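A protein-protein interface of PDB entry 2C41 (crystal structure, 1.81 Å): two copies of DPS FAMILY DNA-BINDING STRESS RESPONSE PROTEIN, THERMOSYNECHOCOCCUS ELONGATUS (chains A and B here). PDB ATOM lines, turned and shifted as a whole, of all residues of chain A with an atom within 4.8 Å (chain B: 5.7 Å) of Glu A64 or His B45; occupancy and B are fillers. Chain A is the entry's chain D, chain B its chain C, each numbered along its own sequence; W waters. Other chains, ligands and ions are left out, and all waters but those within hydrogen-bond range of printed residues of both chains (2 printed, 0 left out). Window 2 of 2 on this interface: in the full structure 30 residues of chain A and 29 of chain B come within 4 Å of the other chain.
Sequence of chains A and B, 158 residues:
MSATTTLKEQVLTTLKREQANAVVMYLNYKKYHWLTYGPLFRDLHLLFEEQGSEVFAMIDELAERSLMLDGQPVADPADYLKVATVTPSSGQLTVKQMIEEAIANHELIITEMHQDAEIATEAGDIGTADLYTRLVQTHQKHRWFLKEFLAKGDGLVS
NZ of Lys B30 is in salt-bridge range of OE1 of Glu B49, 2.8 Å away.
A ring nitrogen (ND1) of His B33 sits at hydrogen-bond distance from the backbone carbonyl oxygen (O) of His B45 (2.7 Å).
NE2 of His B33 lies close to OE1 of Glu B49.
Hydrophobic or aromatic side chains of chain B that line the printed part of chain A: His B33, Trp B34 and His B45.
Of the 9 printed residues of chain A, 4 touch a printed residue of chain B.
Printed residues of chain A that touch a printed residue of chain B: Asp A60, Ala A63, Glu A64 and Leu A67.
Hydrophobic or aromatic side chains of chain A that line the printed part of chain B: Ala A63 and Leu A67.
The side-chain amino group (NZ) of Lys B30 lies within salt-bridge range of the side-chain carboxylate (OD2) of Asp A60.
The side-chain carboxylate (OE2) of Glu A64 is in hydrogen-bond range of a ring nitrogen (NE2) of His B33 (3.1 Å).
The side-chain carboxylate of Asp A60 lies within hydrogen-bond range of the indole nitrogen of Trp B34.
Water W1 lies within hydrogen-bond range of OD1 of Asp A60, NE2 of His B33 and OE2 of Glu A64.
Water W2 lies within hydrogen-bond range of the side-chain carboxylate (OE1) of Glu A64 (2.7 Å) and a ring nitrogen (NE2) of His B45 (2.8 Å).
Glu A64 touches just these residues of chain B: His B33 (3.1 Å), Trp B34 (3.5 Å) and His B45 (3.1 Å).
Of chain A, only Glu A64 (3.1 Å) comes within 4 Å of His B45.
Of the printed residues of chain B, Asp A60 touches Lys B30, His B33 and Trp B34.
Of the printed residues of chain A, Lys B30 touches Asp A60 (2.8 Å).
Printed residues of chain A within 4 Å of Trp B34: Asp A60 (2.9 Å), Ala A63 (3.3 Å), Glu A64 (3.5 Å) and Leu A67 (3.6 Å).
Of the printed residues of chain A, His B33 touches Asp A60 (3.6 Å) and Glu A64 (3.1 Å).
Of the printed residues of chain B, Ala A63 touches Trp B34 (3.3 Å).
Thr B36 touches none of the printed residues of chain A.
The nearest printed residue of chain B that does not touch Glu A64 is Lys B30 (5.7 Å).
The nearest printed residue of chain A that does not touch His B45 is Asp A60 (6.1 Å).
The nearest printed residue of chain A that does not touch His B33 is Leu A67 (6.5 Å).
Asp A60 touches His B33.
CB of Ala A63 touches CE2 of Trp B34, at 3.3 Å.
Glu A64 touches Trp B34.
Glu A64 touches His B45 (OE2 to CE1, 3.1 Å).
Leu A67 touches Trp B34.
No position is printed for both chains.
Of the 8 pairs that touch across the chains among the printed residues, none has its exchanged pair printed and touching as well.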
ATOM      1  N   ASP A  60      18.311 -11.799 -34.083  1.00  0.00           N
ATOM      2  CA  ASP A  60      18.178 -10.351 -33.953  1.00  0.00           C
ATOM      3  C   ASP A  60      18.320  -9.637 -35.302  1.00  0.00           C
ATOM      4  O   ASP A  60      17.597  -8.685 -35.595  1.00  0.00           O
ATOM      5  CB  ASP A  60      19.202  -9.816 -32.947  1.00  0.00           C
ATOM      6  CG  ASP A  60      18.865  -8.417 -32.474  1.00  0.00           C
ATOM      7  OD1 ASP A  60      19.604  -7.476 -32.845  1.00  0.00           O
ATOM      8  OD2 ASP A  60      17.856  -8.261 -31.751  1.00  0.00           O
ATOM      9  N   GLU A  61      19.244 -10.107 -36.134  1.00  0.00           N
ATOM     10  CA  GLU A  61      19.440  -9.500 -37.457  1.00  0.00           C
ATOM     11  C   GLU A  61      18.180  -9.574 -38.317  1.00  0.00           C
ATOM     12  O   GLU A  61      17.766  -8.583 -38.926  1.00  0.00           O
ATOM     13  CB  GLU A  61      20.580 -10.187 -38.202  1.00  0.00           C
ATOM     14  CG  GLU A  61      21.953  -9.926 -37.629  1.00  0.00           C
ATOM     15  CD  GLU A  61      23.015 -10.121 -38.687  1.00  0.00           C
ATOM     16  OE1 GLU A  61      23.633 -11.198 -38.710  1.00  0.00           O
ATOM     17  OE2 GLU A  61      23.199  -9.206 -39.518  1.00  0.00           O
ATOM     18  N   LEU A  62      17.576 -10.757 -38.356  1.00  0.00           N
ATOM     19  CA  LEU A  62      16.380 -10.985 -39.176  1.00  0.00           C
ATOM     20  C   LEU A  62      15.162 -10.279 -38.603  1.00  0.00           C
ATOM     21  O   LEU A  62      14.337  -9.755 -39.355  1.00  0.00           O
ATOM     22  CB  LEU A  62      16.104 -12.480 -39.325  1.00  0.00           C
ATOM     23  CG  LEU A  62      17.149 -13.252 -40.139  1.00  0.00           C
ATOM     24  CD1 LEU A  62      17.054 -14.749 -39.846  1.00  0.00           C
ATOM     25  CD2 LEU A  62      16.994 -12.975 -41.632  1.00  0.00           C
ATOM     26  N   ALA A  63      15.058 -10.254 -37.273  1.00  0.00           N
ATOM     27  CA  ALA A  63      13.952  -9.565 -36.602  1.00  0.00           C
ATOM     28  C   ALA A  63      14.026  -8.059 -36.819  1.00  0.00           C
ATOM     29  O   ALA A  63      13.045  -7.434 -37.217  1.00  0.00           O
ATOM     30  CB  ALA A  63      13.944  -9.883 -35.117  1.00  0.00           C
ATOM     31  N   GLU A  64      15.202  -7.480 -36.597  1.00  0.00           N
ATOM     32  CA  GLU A  64      15.333  -6.031 -36.724  1.00  0.00           C
ATOM     33  C   GLU A  64      15.247  -5.558 -38.169  1.00  0.00           C
ATOM     34  O   GLU A  64      14.828  -4.430 -38.427  1.00  0.00           O
ATOM     35  CB  GLU A  64      16.553  -5.494 -35.955  1.00  0.00           C
ATOM     36  CG  GLU A  64      16.426  -5.794 -34.450  1.00  0.00           C
ATOM     37  CD  GLU A  64      17.269  -4.925 -33.541  1.00  0.00           C
ATOM     38  OE1 GLU A  64      18.293  -4.366 -33.995  1.00  0.00           O
ATOM     39  OE2 GLU A  64      16.904  -4.829 -32.343  1.00  0.00           O
ATOM     40  N   ARG A  65      15.592  -6.430 -39.113  1.00  0.00           N
ATOM     41  CA  ARG A  65      15.399  -6.105 -40.528  1.00  0.00           C
ATOM     42  C   ARG A  65      13.933  -5.764 -40.827  1.00  0.00           C
ATOM     43  O   ARG A  65      13.649  -4.813 -41.560  1.00  0.00           O
ATOM     44  CB  ARG A  65      15.887  -7.230 -41.436  1.00  0.00           C
ATOM     45  CG  ARG A  65      15.949  -6.839 -42.910  1.00  0.00           C
ATOM     46  CD  ARG A  65      17.090  -5.863 -43.214  1.00  0.00           C
ATOM     47  NE  ARG A  65      16.907  -5.263 -44.543  1.00  0.00           N
ATOM     48  CZ  ARG A  65      17.391  -4.083 -44.921  1.00  0.00           C
ATOM     49  NH1 ARG A  65      18.121  -3.354 -44.079  1.00  0.00           N
ATOM     50  NH2 ARG A  65      17.139  -3.626 -46.145  1.00  0.00           N
ATOM     51  N   SER A  66      13.007  -6.527 -40.245  1.00  0.00           N
ATOM     52  CA  SER A  66      11.576  -6.233 -40.382  1.00  0.00           C
ATOM     53  C   SER A  66      11.236  -4.821 -39.914  1.00  0.00           C
ATOM     54  O   SER A  66      10.513  -4.099 -40.597  1.00  0.00           O
ATOM     55  CB  SER A  66      10.739  -7.258 -39.610  1.00  0.00           C
ATOM     56  OG  SER A  66      10.703  -8.495 -40.292  1.00  0.00           O
ATOM     57  N   LEU A  67      11.766  -4.434 -38.753  1.00  0.00           N
ATOM     58  CA  LEU A  67      11.556  -3.091 -38.204  1.00  0.00           C
ATOM     59  C   LEU A  67      12.122  -1.991 -39.106  1.00  0.00           C
ATOM     60  O   LEU A  67      11.505  -0.930 -39.263  1.00  0.00           O
ATOM     61  CB  LEU A  67      12.172  -2.951 -36.807  1.00  0.00           C
ATOM     62  CG  LEU A  67      11.519  -3.503 -35.525  1.00  0.00           C
ATOM     63  CD1 LEU A  67      10.004  -3.341 -35.460  1.00  0.00           C
ATOM     64  CD2 LEU A  67      11.921  -4.912 -35.252  1.00  0.00           C
ATOM     65  N   MET A  68      13.290  -2.243 -39.688  1.00  0.00           N
ATOM     66  CA  MET A  68      13.947  -1.268 -40.568  1.00  0.00           C
ATOM     67  C   MET A  68      13.168  -1.072 -41.863  1.00  0.00           C
ATOM     68  O   MET A  68      13.367  -0.079 -42.566  1.00  0.00           O
ATOM     69  CB  MET A  68      15.388  -1.691 -40.886  1.00  0.00           C
ATOM     70  CG  MET A  68      16.294  -1.678 -39.673  1.00  0.00           C
ATOM     71  SD  MET A  68      17.875  -2.459 -40.046  1.00  0.00           S
ATOM     72  CE  MET A  68      18.085  -3.428 -38.587  1.00  0.00           C
ATOM     73  N   LYS B  30      12.986 -10.252 -25.955  1.00  0.00           N
ATOM     74  CA  LYS B  30      13.294  -9.918 -27.337  1.00  0.00           C
ATOM     75  C   LYS B  30      12.122  -9.178 -27.988  1.00  0.00           C
ATOM     76  O   LYS B  30      12.331  -8.189 -28.696  1.00  0.00           O
ATOM     77  CB  LYS B  30      13.705 -11.159 -28.139  1.00  0.00           C
ATOM     78  CG  LYS B  30      15.095 -11.710 -27.777  1.00  0.00           C
ATOM     79  CD  LYS B  30      16.192 -10.628 -27.726  1.00  0.00           C
ATOM     80  CE  LYS B  30      16.469 -10.022 -29.106  1.00  0.00           C
ATOM     81  NZ  LYS B  30      17.845  -9.452 -29.228  1.00  0.00           N
ATOM     82  N   HIS B  33      12.319  -5.648 -26.617  1.00  0.00           N
ATOM     83  CA  HIS B  33      13.469  -5.038 -27.289  1.00  0.00           C
ATOM     84  C   HIS B  33      13.086  -4.571 -28.701  1.00  0.00           C
ATOM     85  O   HIS B  33      13.348  -3.428 -29.071  1.00  0.00           O
ATOM     86  CB  HIS B  33      14.605  -6.072 -27.330  1.00  0.00           C
ATOM     87  CG  HIS B  33      15.838  -5.633 -28.051  1.00  0.00           C
ATOM     88  ND1 HIS B  33      16.656  -4.621 -27.590  1.00  0.00           N
ATOM     89  CD2 HIS B  33      16.434  -6.122 -29.163  1.00  0.00           C
ATOM     90  CE1 HIS B  33      17.688  -4.491 -28.404  1.00  0.00           C
ATOM     91  NE2 HIS B  33      17.577  -5.390 -29.366  1.00  0.00           N
ATOM     92  N   TRP B  34      12.440  -5.445 -29.473  1.00  0.00           N
ATOM     93  CA  TRP B  34      12.124  -5.125 -30.860  1.00  0.00           C
ATOM     94  C   TRP B  34      10.977  -4.132 -31.021  1.00  0.00           C
ATOM     95  O   TRP B  34      11.002  -3.288 -31.925  1.00  0.00           O
ATOM     96  CB  TRP B  34      11.791  -6.397 -31.640  1.00  0.00           C
ATOM     97  CG  TRP B  34      12.937  -7.367 -31.737  1.00  0.00           C
ATOM     98  CD1 TRP B  34      14.268  -7.065 -31.871  1.00  0.00           C
ATOM     99  CD2 TRP B  34      12.848  -8.792 -31.744  1.00  0.00           C
ATOM    100  NE1 TRP B  34      15.006  -8.216 -31.940  1.00  0.00           N
ATOM    101  CE2 TRP B  34      14.164  -9.292 -31.868  1.00  0.00           C
ATOM    102  CE3 TRP B  34      11.782  -9.700 -31.658  1.00  0.00           C
ATOM    103  CZ2 TRP B  34      14.449 -10.665 -31.903  1.00  0.00           C
ATOM    104  CZ3 TRP B  34      12.067 -11.069 -31.685  1.00  0.00           C
ATOM    105  CH2 TRP B  34      13.389 -11.533 -31.819  1.00  0.00           C
ATOM    106  N   THR B  36       9.511  -2.021 -28.654  1.00  0.00           N
ATOM    107  CA  THR B  36       9.430  -0.809 -27.848  1.00  0.00           C
ATOM    108  C   THR B  36       9.510   0.434 -28.765  1.00  0.00           C
ATOM    109  O   THR B  36      10.038   0.374 -29.884  1.00  0.00           O
ATOM    110  CB  THR B  36      10.441  -0.823 -26.667  1.00  0.00           C
ATOM    111  OG1 THR B  36      10.090   0.188 -25.702  1.00  0.00           O
ATOM    112  CG2 THR B  36      11.866  -0.639 -27.155  1.00  0.00           C
ATOM    113  N   LEU B  40      11.491   7.198 -25.235  1.00  0.00           N
ATOM    114  CA  LEU B  40      12.403   6.439 -24.378  1.00  0.00           C
ATOM    115  C   LEU B  40      13.076   5.299 -25.137  1.00  0.00           C
ATOM    116  O   LEU B  40      13.684   4.408 -24.521  1.00  0.00           O
ATOM    117  CB  LEU B  40      11.652   5.869 -23.165  1.00  0.00           C
ATOM    118  CG  LEU B  40      10.754   6.840 -22.391  1.00  0.00           C
ATOM    119  CD1 LEU B  40      10.012   6.112 -21.267  1.00  0.00           C
ATOM    120  CD2 LEU B  40      11.546   8.029 -21.850  1.00  0.00           C
ATOM    121  N   PHE B  41      12.969   5.322 -26.465  1.00  0.00           N
ATOM    122  CA  PHE B  41      13.366   4.166 -27.263  1.00  0.00           C
ATOM    123  C   PHE B  41      14.766   3.609 -26.966  1.00  0.00           C
ATOM    124  O   PHE B  41      14.905   2.428 -26.655  1.00  0.00           O
ATOM    125  CB  PHE B  41      13.210   4.401 -28.768  1.00  0.00           C
ATOM    126  CG  PHE B  41      13.656   3.225 -29.579  1.00  0.00           C
ATOM    127  CD1 PHE B  41      12.853   2.095 -29.682  1.00  0.00           C
ATOM    128  CD2 PHE B  41      14.915   3.213 -30.177  1.00  0.00           C
ATOM    129  CE1 PHE B  41      13.277   0.979 -30.407  1.00  0.00           C
ATOM    130  CE2 PHE B  41      15.347   2.104 -30.904  1.00  0.00           C
ATOM    131  CZ  PHE B  41      14.527   0.989 -31.027  1.00  0.00           C
ATOM    132  N   ARG B  42      15.800   4.435 -27.073  1.00  0.00           N
ATOM    133  CA  ARG B  42      17.157   3.896 -26.946  1.00  0.00           C
ATOM    134  C   ARG B  42      17.346   3.285 -25.556  1.00  0.00           C
ATOM    135  O   ARG B  42      17.819   2.146 -25.437  1.00  0.00           O
ATOM    136  CB  ARG B  42      18.237   4.950 -27.252  1.00  0.00           C
ATOM    137  CG  ARG B  42      19.665   4.421 -27.107  1.00  0.00           C
ATOM    138  CD  ARG B  42      20.722   5.513 -27.295  1.00  0.00           C
ATOM    139  NE  ARG B  42      22.062   5.063 -26.877  1.00  0.00           N
ATOM    140  CZ  ARG B  42      22.479   4.939 -25.611  1.00  0.00           C
ATOM    141  NH1 ARG B  42      21.673   5.210 -24.587  1.00  0.00           N
ATOM    142  NH2 ARG B  42      23.717   4.530 -25.362  1.00  0.00           N
ATOM    143  N   ASP B  43      16.944   4.032 -24.527  1.00  0.00           N
ATOM    144  CA  ASP B  43      17.080   3.601 -23.129  1.00  0.00           C
ATOM    145  C   ASP B  43      16.401   2.245 -22.904  1.00  0.00           C
ATOM    146  O   ASP B  43      17.005   1.333 -22.344  1.00  0.00           O
ATOM    147  CB  ASP B  43      16.497   4.650 -22.168  1.00  0.00           C
ATOM    148  CG  ASP B  43      17.065   4.543 -20.742  1.00  0.00           C
ATOM    149  OD1 ASP B  43      18.256   4.183 -20.582  1.00  0.00           O
ATOM    150  OD2 ASP B  43      16.330   4.858 -19.773  1.00  0.00           O
ATOM    151  N   LEU B  44      15.154   2.119 -23.348  1.00  0.00           N
ATOM    152  CA  LEU B  44      14.415   0.870 -23.148  1.00  0.00           C
ATOM    153  C   LEU B  44      14.845  -0.266 -24.074  1.00  0.00           C
ATOM    154  O   LEU B  44      14.899  -1.424 -23.656  1.00  0.00           O
ATOM    155  CB  LEU B  44      12.906   1.107 -23.214  1.00  0.00           C
ATOM    156  CG  LEU B  44      12.367   1.693 -21.891  1.00  0.00           C
ATOM    157  CD1 LEU B  44      10.946   2.125 -22.023  1.00  0.00           C
ATOM    158  CD2 LEU B  44      12.495   0.703 -20.725  1.00  0.00           C
ATOM    159  N   HIS B  45      15.165   0.067 -25.322  1.00  0.00           N
ATOM    160  CA  HIS B  45      15.742  -0.903 -26.264  1.00  0.00           C
ATOM    161  C   HIS B  45      16.944  -1.588 -25.591  1.00  0.00           C
ATOM    162  O   HIS B  45      17.070  -2.827 -25.592  1.00  0.00           O
ATOM    163  CB  HIS B  45      16.149  -0.151 -27.539  1.00  0.00           C
ATOM    164  CG  HIS B  45      16.582  -1.025 -28.673  1.00  0.00           C
ATOM    165  ND1 HIS B  45      15.741  -1.935 -29.281  1.00  0.00           N
ATOM    166  CD2 HIS B  45      17.752  -1.080 -29.354  1.00  0.00           C
ATOM    167  CE1 HIS B  45      16.381  -2.525 -30.274  1.00  0.00           C
ATOM    168  NE2 HIS B  45      17.600  -2.021 -30.342  1.00  0.00           N
ATOM    169  N   LEU B  46      17.800  -0.778 -24.970  1.00  0.00           N
ATOM    170  CA  LEU B  46      18.970  -1.297 -24.251  1.00  0.00           C
ATOM    171  C   LEU B  46      18.588  -2.081 -22.997  1.00  0.00           C
ATOM    172  O   LEU B  46      19.126  -3.167 -22.768  1.00  0.00           O
ATOM    173  CB  LEU B  46      19.926  -0.162 -23.877  1.00  0.00           C
ATOM    174  CG  LEU B  46      20.682   0.389 -25.081  1.00  0.00           C
ATOM    175  CD1 LEU B  46      21.425   1.684 -24.747  1.00  0.00           C
ATOM    176  CD2 LEU B  46      21.636  -0.690 -25.610  1.00  0.00           C
ATOM    177  N   LEU B  47      17.676  -1.531 -22.192  1.00  0.00           N
ATOM    178  CA  LEU B  47      17.228  -2.221 -20.982  1.00  0.00           C
ATOM    179  C   LEU B  47      16.753  -3.633 -21.287  1.00  0.00           C
ATOM    180  O   LEU B  47      17.171  -4.595 -20.635  1.00  0.00           O
ATOM    181  CB  LEU B  47      16.117  -1.444 -20.266  1.00  0.00           C
ATOM    182  CG  LEU B  47      15.564  -2.161 -19.028  1.00  0.00           C
ATOM    183  CD1 LEU B  47      16.474  -1.979 -17.814  1.00  0.00           C
ATOM    184  CD2 LEU B  47      14.158  -1.657 -18.743  1.00  0.00           C
ATOM    185  N   PHE B  48      15.886  -3.758 -22.287  1.00  0.00           N
ATOM    186  CA  PHE B  48      15.314  -5.052 -22.634  1.00  0.00           C
ATOM    187  C   PHE B  48      16.372  -6.030 -23.138  1.00  0.00           C
ATOM    188  O   PHE B  48      16.311  -7.213 -22.831  1.00  0.00           O
ATOM    189  CB  PHE B  48      14.170  -4.885 -23.637  1.00  0.00           C
ATOM    190  CG  PHE B  48      12.975  -4.142 -23.073  1.00  0.00           C
ATOM    191  CD1 PHE B  48      12.363  -3.120 -23.795  1.00  0.00           C
ATOM    192  CD2 PHE B  48      12.459  -4.488 -21.820  1.00  0.00           C
ATOM    193  CE1 PHE B  48      11.255  -2.436 -23.272  1.00  0.00           C
ATOM    194  CE2 PHE B  48      11.348  -3.819 -21.284  1.00  0.00           C
ATOM    195  CZ  PHE B  48      10.747  -2.793 -22.004  1.00  0.00           C
ATOM    196  N   GLU B  49      17.351  -5.525 -23.876  1.00  0.00           N
ATOM    197  CA  GLU B  49      18.452  -6.369 -24.338  1.00  0.00           C
ATOM    198  C   GLU B  49      19.332  -6.812 -23.169  1.00  0.00           C
ATOM    199  O   GLU B  49      19.727  -7.971 -23.087  1.00  0.00           O
ATOM    200  CB  GLU B  49      19.270  -5.648 -25.417  1.00  0.00           C
ATOM    201  CG  GLU B  49      20.347  -6.531 -26.047  1.00  0.00           C
ATOM    202  CD  GLU B  49      19.812  -7.606 -27.002  1.00  0.00           C
ATOM    203  OE1 GLU B  49      18.584  -7.834 -27.108  1.00  0.00           O
ATOM    204  OE2 GLU B  49      20.649  -8.249 -27.660  1.00  0.00           O
ATOM    205  N   GLU B  50      19.616  -5.885 -22.253  1.00  0.00           N
ATOM    206  CA  GLU B  50      20.500  -6.167 -21.128  1.00  0.00           C
ATOM    207  C   GLU B  50      19.894  -7.203 -20.192  1.00  0.00           C
ATOM    208  O   GLU B  50      20.534  -8.210 -19.865  1.00  0.00           O
ATOM    209  CB  GLU B  50      20.828  -4.877 -20.379  1.00  0.00           C
ATOM    210  CG  GLU B  50      21.762  -3.974 -21.157  1.00  0.00           C
ATOM    211  CD  GLU B  50      21.770  -2.545 -20.652  1.00  0.00           C
ATOM    212  OE1 GLU B  50      20.842  -2.146 -19.907  1.00  0.00           O
ATOM    213  OE2 GLU B  50      22.699  -1.812 -21.032  1.00  0.00           O
HETATM  214  O   HOH W   1      19.643  -5.548 -31.123  1.00  0.00           O
HETATM  215  O   HOH W   2      19.497  -2.862 -32.174  1.00  0.00           O
